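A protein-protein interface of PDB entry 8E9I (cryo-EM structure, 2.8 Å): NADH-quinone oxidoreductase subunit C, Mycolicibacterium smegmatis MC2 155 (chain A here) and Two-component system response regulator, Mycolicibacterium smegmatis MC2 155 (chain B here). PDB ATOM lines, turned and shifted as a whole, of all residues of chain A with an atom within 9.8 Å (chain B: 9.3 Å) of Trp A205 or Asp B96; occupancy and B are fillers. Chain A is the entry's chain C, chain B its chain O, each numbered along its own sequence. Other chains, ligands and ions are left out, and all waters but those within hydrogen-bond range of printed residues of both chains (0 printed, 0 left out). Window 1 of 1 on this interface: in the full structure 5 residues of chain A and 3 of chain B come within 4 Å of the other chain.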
ATOM      1  N   TYR A 183     -10.084 -11.438  -8.222  1.00  0.00           N
ATOM      2  CA  TYR A 183     -11.509 -11.693  -8.378  1.00  0.00           C
ATOM      3  C   TYR A 183     -12.098 -10.761  -9.419  1.00  0.00           C
ATOM      4  O   TYR A 183     -12.678 -11.206 -10.415  1.00  0.00           O
ATOM      5  CB  TYR A 183     -12.245 -11.521  -7.051  1.00  0.00           C
ATOM      6  CG  TYR A 183     -13.711 -11.234  -7.259  1.00  0.00           C
ATOM      7  CD1 TYR A 183     -14.534 -12.159  -7.876  1.00  0.00           C
ATOM      8  CD2 TYR A 183     -14.267 -10.029  -6.869  1.00  0.00           C
ATOM      9  CE1 TYR A 183     -15.868 -11.899  -8.084  1.00  0.00           C
ATOM     10  CE2 TYR A 183     -15.602  -9.762  -7.075  1.00  0.00           C
ATOM     11  CZ  TYR A 183     -16.394 -10.699  -7.683  1.00  0.00           C
ATOM     12  OH  TYR A 183     -17.727 -10.439  -7.889  1.00  0.00           O
ATOM     13  N   ASP A 184     -11.883  -9.458  -9.244  1.00  0.00           N
ATOM     14  CA  ASP A 184     -12.466  -8.477 -10.148  1.00  0.00           C
ATOM     15  C   ASP A 184     -12.135  -8.818 -11.589  1.00  0.00           C
ATOM     16  O   ASP A 184     -12.963  -8.660 -12.492  1.00  0.00           O
ATOM     17  CB  ASP A 184     -11.938  -7.088  -9.806  1.00  0.00           C
ATOM     18  CG  ASP A 184     -12.685  -6.000 -10.518  1.00  0.00           C
ATOM     19  OD1 ASP A 184     -13.721  -6.301 -11.139  1.00  0.00           O
ATOM     20  OD2 ASP A 184     -12.230  -4.843 -10.466  1.00  0.00           O
ATOM     21  N   PHE A 185     -10.925  -9.308 -11.812  1.00  0.00           N
ATOM     22  CA  PHE A 185     -10.434  -9.523 -13.160  1.00  0.00           C
ATOM     23  C   PHE A 185     -10.732 -10.924 -13.666  1.00  0.00           C
ATOM     24  O   PHE A 185     -10.730 -11.147 -14.880  1.00  0.00           O
ATOM     25  CB  PHE A 185      -8.934  -9.259 -13.175  1.00  0.00           C
ATOM     26  CG  PHE A 185      -8.573  -7.809 -13.103  1.00  0.00           C
ATOM     27  CD1 PHE A 185      -9.546  -6.827 -13.131  1.00  0.00           C
ATOM     28  CD2 PHE A 185      -7.255  -7.428 -12.965  1.00  0.00           C
ATOM     29  CE1 PHE A 185      -9.210  -5.502 -13.055  1.00  0.00           C
ATOM     30  CE2 PHE A 185      -6.915  -6.100 -12.881  1.00  0.00           C
ATOM     31  CZ  PHE A 185      -7.898  -5.137 -12.927  1.00  0.00           C
ATOM     32  N   PHE A 186     -10.997 -11.874 -12.770  1.00  0.00           N
ATOM     33  CA  PHE A 186     -11.206 -13.253 -13.179  1.00  0.00           C
ATOM     34  C   PHE A 186     -12.434 -13.897 -12.574  1.00  0.00           C
ATOM     35  O   PHE A 186     -12.905 -14.902 -13.114  1.00  0.00           O
ATOM     36  CB  PHE A 186      -9.985 -14.109 -12.819  1.00  0.00           C
ATOM     37  CG  PHE A 186      -8.743 -13.715 -13.548  1.00  0.00           C
ATOM     38  CD1 PHE A 186      -8.513 -14.159 -14.833  1.00  0.00           C
ATOM     39  CD2 PHE A 186      -7.808 -12.897 -12.951  1.00  0.00           C
ATOM     40  CE1 PHE A 186      -7.375 -13.795 -15.508  1.00  0.00           C
ATOM     41  CE2 PHE A 186      -6.667 -12.533 -13.622  1.00  0.00           C
ATOM     42  CZ  PHE A 186      -6.452 -12.981 -14.903  1.00  0.00           C
ATOM     43  N   ARG A 198     -14.913  -5.536  -5.836  1.00  0.00           N
ATOM     44  CA  ARG A 198     -14.076  -5.102  -6.938  1.00  0.00           C
ATOM     45  C   ARG A 198     -13.223  -3.919  -6.503  1.00  0.00           C
ATOM     46  O   ARG A 198     -13.685  -3.000  -5.823  1.00  0.00           O
ATOM     47  CB  ARG A 198     -14.928  -4.719  -8.141  1.00  0.00           C
ATOM     48  CG  ARG A 198     -15.612  -5.890  -8.796  1.00  0.00           C
ATOM     49  CD  ARG A 198     -16.387  -5.451 -10.005  1.00  0.00           C
ATOM     50  NE  ARG A 198     -17.102  -6.558 -10.625  1.00  0.00           N
ATOM     51  CZ  ARG A 198     -16.702  -7.209 -11.709  1.00  0.00           C
ATOM     52  NH1 ARG A 198     -15.571  -6.906 -12.326  1.00  0.00           N
ATOM     53  NH2 ARG A 198     -17.459  -8.189 -12.192  1.00  0.00           N
ATOM     54  N   ILE A 199     -11.955  -3.953  -6.899  1.00  0.00           N
ATOM     55  CA  ILE A 199     -11.013  -2.930  -6.470  1.00  0.00           C
ATOM     56  C   ILE A 199     -10.696  -2.012  -7.642  1.00  0.00           C
ATOM     57  O   ILE A 199     -10.670  -0.787  -7.492  1.00  0.00           O
ATOM     58  CB  ILE A 199      -9.741  -3.565  -5.879  1.00  0.00           C
ATOM     59  CG1 ILE A 199      -8.841  -2.490  -5.278  1.00  0.00           C
ATOM     60  CG2 ILE A 199      -8.983  -4.351  -6.929  1.00  0.00           C
ATOM     61  CD1 ILE A 199      -7.784  -3.041  -4.364  1.00  0.00           C
ATOM     62  N   GLU A 200     -10.479  -2.590  -8.823  1.00  0.00           N
ATOM     63  CA  GLU A 200     -10.127  -1.810 -10.005  1.00  0.00           C
ATOM     64  C   GLU A 200     -11.363  -1.324 -10.753  1.00  0.00           C
ATOM     65  O   GLU A 200     -11.473  -0.138 -11.074  1.00  0.00           O
ATOM     66  CB  GLU A 200      -9.236  -2.638 -10.938  1.00  0.00           C
ATOM     67  CG  GLU A 200      -7.845  -2.898 -10.388  1.00  0.00           C
ATOM     68  CD  GLU A 200      -7.011  -1.648 -10.300  1.00  0.00           C
ATOM     69  OE1 GLU A 200      -7.316  -0.680 -11.015  1.00  0.00           O
ATOM     70  OE2 GLU A 200      -6.050  -1.633  -9.509  1.00  0.00           O
ATOM     71  N   MET A 201     -12.293  -2.225 -11.037  1.00  0.00           N
ATOM     72  CA  MET A 201     -13.445  -1.884 -11.846  1.00  0.00           C
ATOM     73  C   MET A 201     -14.609  -1.441 -10.966  1.00  0.00           C
ATOM     74  O   MET A 201     -14.654  -1.748  -9.774  1.00  0.00           O
ATOM     75  CB  MET A 201     -13.858  -3.081 -12.692  1.00  0.00           C
ATOM     76  CG  MET A 201     -12.878  -3.438 -13.801  1.00  0.00           C
ATOM     77  SD  MET A 201     -12.196  -2.024 -14.686  1.00  0.00           S
ATOM     78  CE  MET A 201     -13.511  -1.658 -15.836  1.00  0.00           C
ATOM     79  N   PRO A 202     -15.569  -0.711 -11.530  1.00  0.00           N
ATOM     80  CA  PRO A 202     -16.717  -0.273 -10.733  1.00  0.00           C
ATOM     81  C   PRO A 202     -17.517  -1.456 -10.213  1.00  0.00           C
ATOM     82  O   PRO A 202     -17.589  -2.511 -10.845  1.00  0.00           O
ATOM     83  CB  PRO A 202     -17.538   0.563 -11.720  1.00  0.00           C
ATOM     84  CG  PRO A 202     -16.579   0.957 -12.772  1.00  0.00           C
ATOM     85  CD  PRO A 202     -15.625  -0.179 -12.899  1.00  0.00           C
ATOM     86  N   ASP A 203     -18.127  -1.267  -9.043  1.00  0.00           N
ATOM     87  CA  ASP A 203     -18.886  -2.350  -8.427  1.00  0.00           C
ATOM     88  C   ASP A 203     -20.001  -2.838  -9.338  1.00  0.00           C
ATOM     89  O   ASP A 203     -20.352  -4.021  -9.310  1.00  0.00           O
ATOM     90  CB  ASP A 203     -19.458  -1.890  -7.090  1.00  0.00           C
ATOM     91  N   ASP A 204     -20.560  -1.952 -10.156  1.00  0.00           N
ATOM     92  CA  ASP A 204     -21.648  -2.311 -11.053  1.00  0.00           C
ATOM     93  C   ASP A 204     -21.157  -2.873 -12.378  1.00  0.00           C
ATOM     94  O   ASP A 204     -21.978  -3.153 -13.255  1.00  0.00           O
ATOM     95  CB  ASP A 204     -22.536  -1.089 -11.307  1.00  0.00           C
ATOM     96  N   TRP A 205     -19.852  -3.033 -12.552  1.00  0.00           N
ATOM     97  CA  TRP A 205     -19.323  -3.536 -13.809  1.00  0.00           C
ATOM     98  C   TRP A 205     -19.729  -4.986 -14.028  1.00  0.00           C
ATOM     99  O   TRP A 205     -19.744  -5.799 -13.100  1.00  0.00           O
ATOM    100  CB  TRP A 205     -17.804  -3.418 -13.826  1.00  0.00           C
ATOM    101  CG  TRP A 205     -17.237  -3.510 -15.190  1.00  0.00           C
ATOM    102  CD1 TRP A 205     -16.737  -4.620 -15.796  1.00  0.00           C
ATOM    103  CD2 TRP A 205     -17.114  -2.446 -16.135  1.00  0.00           C
ATOM    104  NE1 TRP A 205     -16.305  -4.313 -17.061  1.00  0.00           N
ATOM    105  CE2 TRP A 205     -16.526  -2.982 -17.292  1.00  0.00           C
ATOM    106  CE3 TRP A 205     -17.442  -1.091 -16.112  1.00  0.00           C
ATOM    107  CZ2 TRP A 205     -16.260  -2.210 -18.415  1.00  0.00           C
ATOM    108  CZ3 TRP A 205     -17.177  -0.328 -17.225  1.00  0.00           C
ATOM    109  CH2 TRP A 205     -16.594  -0.887 -18.362  1.00  0.00           C
ATOM    110  N   GLU A 206     -20.052  -5.308 -15.278  1.00  0.00           N
ATOM    111  CA  GLU A 206     -20.470  -6.650 -15.662  1.00  0.00           C
ATOM    112  C   GLU A 206     -19.327  -7.376 -16.354  1.00  0.00           C
ATOM    113  O   GLU A 206     -18.698  -6.837 -17.266  1.00  0.00           O
ATOM    114  CB  GLU A 206     -21.687  -6.598 -16.588  1.00  0.00           C
ATOM    115  N   GLY A 207     -19.077  -8.606 -15.925  1.00  0.00           N
ATOM    116  CA  GLY A 207     -18.006  -9.399 -16.481  1.00  0.00           C
ATOM    117  C   GLY A 207     -16.702  -9.193 -15.727  1.00  0.00           C
ATOM    118  O   GLY A 207     -16.558  -8.306 -14.891  1.00  0.00           O
ATOM    119  N   HIS A 208     -15.738 -10.054 -16.047  1.00  0.00           N
ATOM    120  CA  HIS A 208     -14.411 -10.027 -15.434  1.00  0.00           C
ATOM    121  C   HIS A 208     -13.392  -9.835 -16.546  1.00  0.00           C
ATOM    122  O   HIS A 208     -13.081 -10.792 -17.275  1.00  0.00           O
ATOM    123  CB  HIS A 208     -14.140 -11.305 -14.657  1.00  0.00           C
ATOM    124  CG  HIS A 208     -15.028 -11.482 -13.470  1.00  0.00           C
ATOM    125  ND1 HIS A 208     -14.946 -10.680 -12.354  1.00  0.00           N
ATOM    126  CD2 HIS A 208     -16.020 -12.367 -13.227  1.00  0.00           C
ATOM    127  CE1 HIS A 208     -15.850 -11.065 -11.472  1.00  0.00           C
ATOM    128  NE2 HIS A 208     -16.515 -12.087 -11.978  1.00  0.00           N
ATOM    129  N   PRO A 209     -12.848  -8.629 -16.712  1.00  0.00           N
ATOM    130  CA  PRO A 209     -12.155  -8.319 -17.969  1.00  0.00           C
ATOM    131  C   PRO A 209     -10.993  -9.232 -18.315  1.00  0.00           C
ATOM    132  O   PRO A 209     -10.843  -9.580 -19.492  1.00  0.00           O
ATOM    133  CB  PRO A 209     -11.689  -6.879 -17.755  1.00  0.00           C
ATOM    134  CG  PRO A 209     -12.635  -6.325 -16.787  1.00  0.00           C
ATOM    135  CD  PRO A 209     -12.961  -7.440 -15.855  1.00  0.00           C
ATOM    136  N   GLN A 210     -10.168  -9.641 -17.359  1.00  0.00           N
ATOM    137  CA  GLN A 210      -8.985 -10.407 -17.727  1.00  0.00           C
ATOM    138  C   GLN A 210      -9.308 -11.817 -18.200  1.00  0.00           C
ATOM    139  O   GLN A 210      -8.403 -12.507 -18.676  1.00  0.00           O
ATOM    140  CB  GLN A 210      -7.998 -10.470 -16.566  1.00  0.00           C
ATOM    141  CG  GLN A 210      -7.414  -9.118 -16.196  1.00  0.00           C
ATOM    142  CD  GLN A 210      -6.482  -8.585 -17.255  1.00  0.00           C
ATOM    143  OE1 GLN A 210      -6.022  -9.326 -18.120  1.00  0.00           O
ATOM    144  NE2 GLN A 210      -6.196  -7.292 -17.194  1.00  0.00           N
ATOM    145  N   TYR A 214     -14.141 -12.503 -22.009  1.00  0.00           N
ATOM    146  CA  TYR A 214     -14.509 -11.094 -22.030  1.00  0.00           C
ATOM    147  C   TYR A 214     -13.914 -10.420 -23.258  1.00  0.00           C
ATOM    148  O   TYR A 214     -12.694 -10.481 -23.450  1.00  0.00           O
ATOM    149  CB  TYR A 214     -14.007 -10.416 -20.767  1.00  0.00           C
ATOM    150  CG  TYR A 214     -14.497  -9.004 -20.566  1.00  0.00           C
ATOM    151  CD1 TYR A 214     -13.797  -7.924 -21.080  1.00  0.00           C
ATOM    152  CD2 TYR A 214     -15.645  -8.748 -19.836  1.00  0.00           C
ATOM    153  CE1 TYR A 214     -14.236  -6.633 -20.882  1.00  0.00           C
ATOM    154  CE2 TYR A 214     -16.092  -7.464 -19.634  1.00  0.00           C
ATOM    155  CZ  TYR A 214     -15.386  -6.410 -20.158  1.00  0.00           C
ATOM    156  OH  TYR A 214     -15.835  -5.127 -19.952  1.00  0.00           O
ATOM    157  N   PRO A 215     -14.710  -9.771 -24.101  1.00  0.00           N
ATOM    158  CA  PRO A 215     -14.141  -9.117 -25.282  1.00  0.00           C
ATOM    159  C   PRO A 215     -13.278  -7.933 -24.890  1.00  0.00           C
ATOM    160  O   PRO A 215     -13.475  -7.298 -23.854  1.00  0.00           O
ATOM    161  CB  PRO A 215     -15.375  -8.673 -26.069  1.00  0.00           C
ATOM    162  CG  PRO A 215     -16.404  -8.457 -25.033  1.00  0.00           C
ATOM    163  CD  PRO A 215     -16.151  -9.498 -23.974  1.00  0.00           C
ATOM    164  N   LEU A 216     -12.304  -7.633 -25.749  1.00  0.00           N
ATOM    165  CA  LEU A 216     -11.372  -6.555 -25.446  1.00  0.00           C
ATOM    166  C   LEU A 216     -12.089  -5.231 -25.240  1.00  0.00           C
ATOM    167  O   LEU A 216     -11.575  -4.354 -24.543  1.00  0.00           O
ATOM    168  CB  LEU A 216     -10.337  -6.424 -26.557  1.00  0.00           C
ATOM    169  CG  LEU A 216      -9.297  -5.322 -26.359  1.00  0.00           C
ATOM    170  CD1 LEU A 216      -8.513  -5.535 -25.082  1.00  0.00           C
ATOM    171  CD2 LEU A 216      -8.362  -5.258 -27.548  1.00  0.00           C
ATOM    172  N   GLY A 217     -13.264  -5.064 -25.834  1.00  0.00           N
ATOM    173  CA  GLY A 217     -14.014  -3.840 -25.647  1.00  0.00           C
ATOM    174  C   GLY A 217     -13.355  -2.601 -26.204  1.00  0.00           C
ATOM    175  O   GLY A 217     -13.481  -1.527 -25.615  1.00  0.00           O
ATOM    176  N   GLY A 218     -12.651  -2.719 -27.324  1.00  0.00           N
ATOM    177  CA  GLY A 218     -12.112  -1.564 -28.002  1.00  0.00           C
ATOM    178  C   GLY A 218     -13.091  -0.993 -29.004  1.00  0.00           C
ATOM    179  O   GLY A 218     -14.186  -1.509 -29.221  1.00  0.00           O
ATOM    180  N   ILE A 219     -12.679   0.102 -29.633  1.00  0.00           N
ATOM    181  CA  ILE A 219     -13.491   0.736 -30.666  1.00  0.00           C
ATOM    182  C   ILE A 219     -12.638   0.921 -31.915  1.00  0.00           C
ATOM    183  O   ILE A 219     -11.407   0.997 -31.812  1.00  0.00           O
ATOM    184  CB  ILE A 219     -14.070   2.072 -30.180  1.00  0.00           C
ATOM    185  CG1 ILE A 219     -12.957   3.078 -29.898  1.00  0.00           C
ATOM    186  CG2 ILE A 219     -14.885   1.861 -28.933  1.00  0.00           C
ATOM    187  CD1 ILE A 219     -13.469   4.457 -29.630  1.00  0.00           C
ATOM    188  N   MET B  72     -22.910  11.666 -24.152  1.00  0.00           N
ATOM    189  CA  MET B  72     -23.064  11.315 -22.744  1.00  0.00           C
ATOM    190  C   MET B  72     -22.729  12.497 -21.847  1.00  0.00           C
ATOM    191  O   MET B  72     -23.444  12.773 -20.874  1.00  0.00           O
ATOM    192  CB  MET B  72     -22.184  10.117 -22.408  1.00  0.00           C
ATOM    193  CG  MET B  72     -22.616   8.849 -23.104  1.00  0.00           C
ATOM    194  SD  MET B  72     -21.603   7.444 -22.646  1.00  0.00           S
ATOM    195  CE  MET B  72     -20.112   7.831 -23.553  1.00  0.00           C
ATOM    196  N   THR B  92     -24.552   4.812 -28.107  1.00  0.00           N
ATOM    197  CA  THR B  92     -23.241   4.442 -27.596  1.00  0.00           C
ATOM    198  C   THR B  92     -22.450   3.754 -28.697  1.00  0.00           C
ATOM    199  O   THR B  92     -22.965   2.855 -29.369  1.00  0.00           O
ATOM    200  CB  THR B  92     -23.363   3.526 -26.378  1.00  0.00           C
ATOM    201  OG1 THR B  92     -23.932   2.274 -26.770  1.00  0.00           O
ATOM    202  CG2 THR B  92     -24.245   4.166 -25.324  1.00  0.00           C
ATOM    203  N   GLY B  93     -21.202   4.178 -28.876  1.00  0.00           N
ATOM    204  CA  GLY B  93     -20.337   3.594 -29.876  1.00  0.00           C
ATOM    205  C   GLY B  93     -19.670   2.307 -29.460  1.00  0.00           C
ATOM    206  O   GLY B  93     -18.870   1.764 -30.226  1.00  0.00           O
ATOM    207  N   ARG B  94     -19.975   1.801 -28.270  1.00  0.00           N
ATOM    208  CA  ARG B  94     -19.294   0.631 -27.740  1.00  0.00           C
ATOM    209  C   ARG B  94     -20.180  -0.025 -26.695  1.00  0.00           C
ATOM    210  O   ARG B  94     -20.892   0.648 -25.948  1.00  0.00           O
ATOM    211  CB  ARG B  94     -17.942   1.019 -27.145  1.00  0.00           C
ATOM    212  CG  ARG B  94     -17.277  -0.079 -26.366  1.00  0.00           C
ATOM    213  CD  ARG B  94     -15.859   0.281 -25.995  1.00  0.00           C
ATOM    214  NE  ARG B  94     -15.773   1.568 -25.320  1.00  0.00           N
ATOM    215  CZ  ARG B  94     -14.758   1.942 -24.556  1.00  0.00           C
ATOM    216  NH1 ARG B  94     -13.725   1.146 -24.340  1.00  0.00           N
ATOM    217  NH2 ARG B  94     -14.783   3.143 -23.989  1.00  0.00           N
ATOM    218  N   ALA B  95     -20.132  -1.355 -26.657  1.00  0.00           N
ATOM    219  CA  ALA B  95     -20.929  -2.089 -25.683  1.00  0.00           C
ATOM    220  C   ALA B  95     -20.451  -1.821 -24.263  1.00  0.00           C
ATOM    221  O   ALA B  95     -21.265  -1.706 -23.341  1.00  0.00           O
ATOM    222  CB  ALA B  95     -20.881  -3.583 -25.986  1.00  0.00           C
ATOM    223  N   ASP B  96     -19.135  -1.727 -24.070  1.00  0.00           N
ATOM    224  CA  ASP B  96     -18.588  -1.388 -22.765  1.00  0.00           C
ATOM    225  C   ASP B  96     -18.953   0.021 -22.330  1.00  0.00           C
ATOM    226  O   ASP B  96     -18.807   0.339 -21.147  1.00  0.00           O
ATOM    227  CB  ASP B  96     -17.067  -1.538 -22.781  1.00  0.00           C
ATOM    228  N   ASP B  97     -19.413   0.872 -23.248  1.00  0.00           N
ATOM    229  CA  ASP B  97     -19.828   2.219 -22.877  1.00  0.00           C
ATOM    230  C   ASP B  97     -21.129   2.226 -22.088  1.00  0.00           C
ATOM    231  O   ASP B  97     -21.508   3.273 -21.552  1.00  0.00           O
ATOM    232  CB  ASP B  97     -19.977   3.084 -24.128  1.00  0.00           C
ATOM    233  N   ALA B  98     -21.812   1.087 -21.994  1.00  0.00           N
ATOM    234  CA  ALA B  98     -23.092   1.017 -21.304  1.00  0.00           C
ATOM    235  C   ALA B  98     -22.985   1.617 -19.915  1.00  0.00           C
ATOM    236  O   ALA B  98     -23.862   2.378 -19.495  1.00  0.00           O
ATOM    237  CB  ALA B  98     -23.574  -0.429 -21.205  1.00  0.00           C
ATOM    238  N   TRP B  99     -21.910   1.292 -19.198  1.00  0.00           N
ATOM    239  CA  TRP B  99     -21.760   1.821 -17.851  1.00  0.00           C
ATOM    240  C   TRP B  99     -21.818   3.340 -17.863  1.00  0.00           C
ATOM    241  O   TRP B  99     -22.578   3.942 -17.100  1.00  0.00           O
ATOM    242  CB  TRP B  99     -20.452   1.325 -17.240  1.00  0.00           C
ATOM    243  CG  TRP B  99     -20.324   1.608 -15.783  1.00  0.00           C
ATOM    244  CD1 TRP B  99     -20.866   0.887 -14.768  1.00  0.00           C
ATOM    245  CD2 TRP B  99     -19.600   2.675 -15.175  1.00  0.00           C
ATOM    246  NE1 TRP B  99     -20.532   1.441 -13.562  1.00  0.00           N
ATOM    247  CE2 TRP B  99     -19.751   2.543 -13.786  1.00  0.00           C
ATOM    248  CE3 TRP B  99     -18.838   3.734 -15.671  1.00  0.00           C
ATOM    249  CZ2 TRP B  99     -19.172   3.426 -12.887  1.00  0.00           C
ATOM    250  CZ3 TRP B  99     -18.264   4.608 -14.779  1.00  0.00           C
ATOM    251  CH2 TRP B  99     -18.434   4.452 -13.403  1.00  0.00           C
ATOM    252  N   LEU B 100     -21.063   3.978 -18.758  1.00  0.00           N
ATOM    253  CA  LEU B 100     -21.142   5.429 -18.857  1.00  0.00           C
ATOM    254  C   LEU B 100     -22.541   5.885 -19.230  1.00  0.00           C
ATOM    255  O   LEU B 100     -23.021   6.895 -18.702  1.00  0.00           O
ATOM    256  CB  LEU B 100     -20.125   5.952 -19.865  1.00  0.00           C
ATOM    257  CG  LEU B 100     -18.691   5.979 -19.347  1.00  0.00           C
ATOM    258  CD1 LEU B 100     -17.755   6.489 -20.418  1.00  0.00           C
ATOM    259  CD2 LEU B 100     -18.586   6.843 -18.102  1.00  0.00           C
ATOM    260  N   ALA B 101     -23.217   5.157 -20.114  1.00  0.00           N
ATOM    261  CA  ALA B 101     -24.601   5.496 -20.416  1.00  0.00           C
ATOM    262  C   ALA B 101     -25.461   5.415 -19.163  1.00  0.00           C
ATOM    263  O   ALA B 101     -26.373   6.228 -18.973  1.00  0.00           O
ATOM    264  CB  ALA B 101     -25.140   4.575 -21.505  1.00  0.00           C
ATOM    265  N   LYS B 102     -25.187   4.444 -18.290  1.00  0.00           N
ATOM    266  CA  LYS B 102     -25.874   4.420 -17.005  1.00  0.00           C
ATOM    267  C   LYS B 102     -25.549   5.670 -16.200  1.00  0.00           C
ATOM    268  O   LYS B 102     -26.435   6.262 -15.574  1.00  0.00           O
ATOM    269  CB  LYS B 102     -25.497   3.161 -16.227  1.00  0.00           C
ATOM    270  N   PRO B 111     -27.019   0.985 -28.702  1.00  0.00           N
ATOM    271  CA  PRO B 111     -25.658   0.868 -29.236  1.00  0.00           C
ATOM    272  C   PRO B 111     -25.602   1.133 -30.731  1.00  0.00           C
ATOM    273  O   PRO B 111     -26.544   0.842 -31.470  1.00  0.00           O
ATOM    274  CB  PRO B 111     -25.277  -0.584 -28.919  1.00  0.00           C
ATOM    275  CG  PRO B 111     -26.237  -1.017 -27.867  1.00  0.00           C
ATOM    276  CD  PRO B 111     -27.500  -0.300 -28.172  1.00  0.00           C
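NH1 of Arg B94 lies within hydrogen-bond range of O of Gly A217.
Trp A205 touches just these residues of chain B: Asp B96 (3.8 Å) and Trp B99 (3.7 Å). Asp B96 touches just one residue of chain A: Trp A205. Printed residues of chain B within 4 Å of Asp A204: Trp B99 (3.9 Å). No residue of chain B comes within 4 Å of Glu A206. Of chain A, only Gly A217 (3.0 Å) and Ile A219 (3.5 Å) come within 4 Å of Arg B94. Ala B95 touches none of the printed residues of chain A. No residue of chain A comes within 4 Å of Asp B97. Ala B98 touches none of the printed residues of chain A. Printed residues of chain A within 4 Å of Trp B99: Pro A202, Asp A204 and Trp A205. Of the printed residues of chain B, Gly A217 touches Arg B94. Of the printed residues of chain B, Ile A219 touches Arg B94. Ala B101 touches none of the printed residues of chain A. Leu B100 touches none of the printed residues of chain A. The nearest residue of chain A that does not touch Asp B96 is Gly A217 (4.6 Å). The nearest printed residue of chain A that does not touch Trp B99 is Asp A203 (5.8 Å).
Among the printed residues, pairs that only touch across the chains: Pro A202 with Trp B99 (3.5 Å), Asp A204 with Trp B99 (3.9 Å), Trp A205 with Asp B96 (3.8 Å), Trp A205 with Trp B99 (3.7 Å) and Ile A219 with Arg B94 (3.5 Å).
The guanidinium group (NH2) of Arg A198 is in hydrogen-bond range of the backbone carbonyl oxygen (O) of Trp A205, 3.4 Å away. NE1 of Trp A205 sits at hydrogen-bond distance from OH of Tyr A214.
Among the printed residues, 6 pairs touch across the chains.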
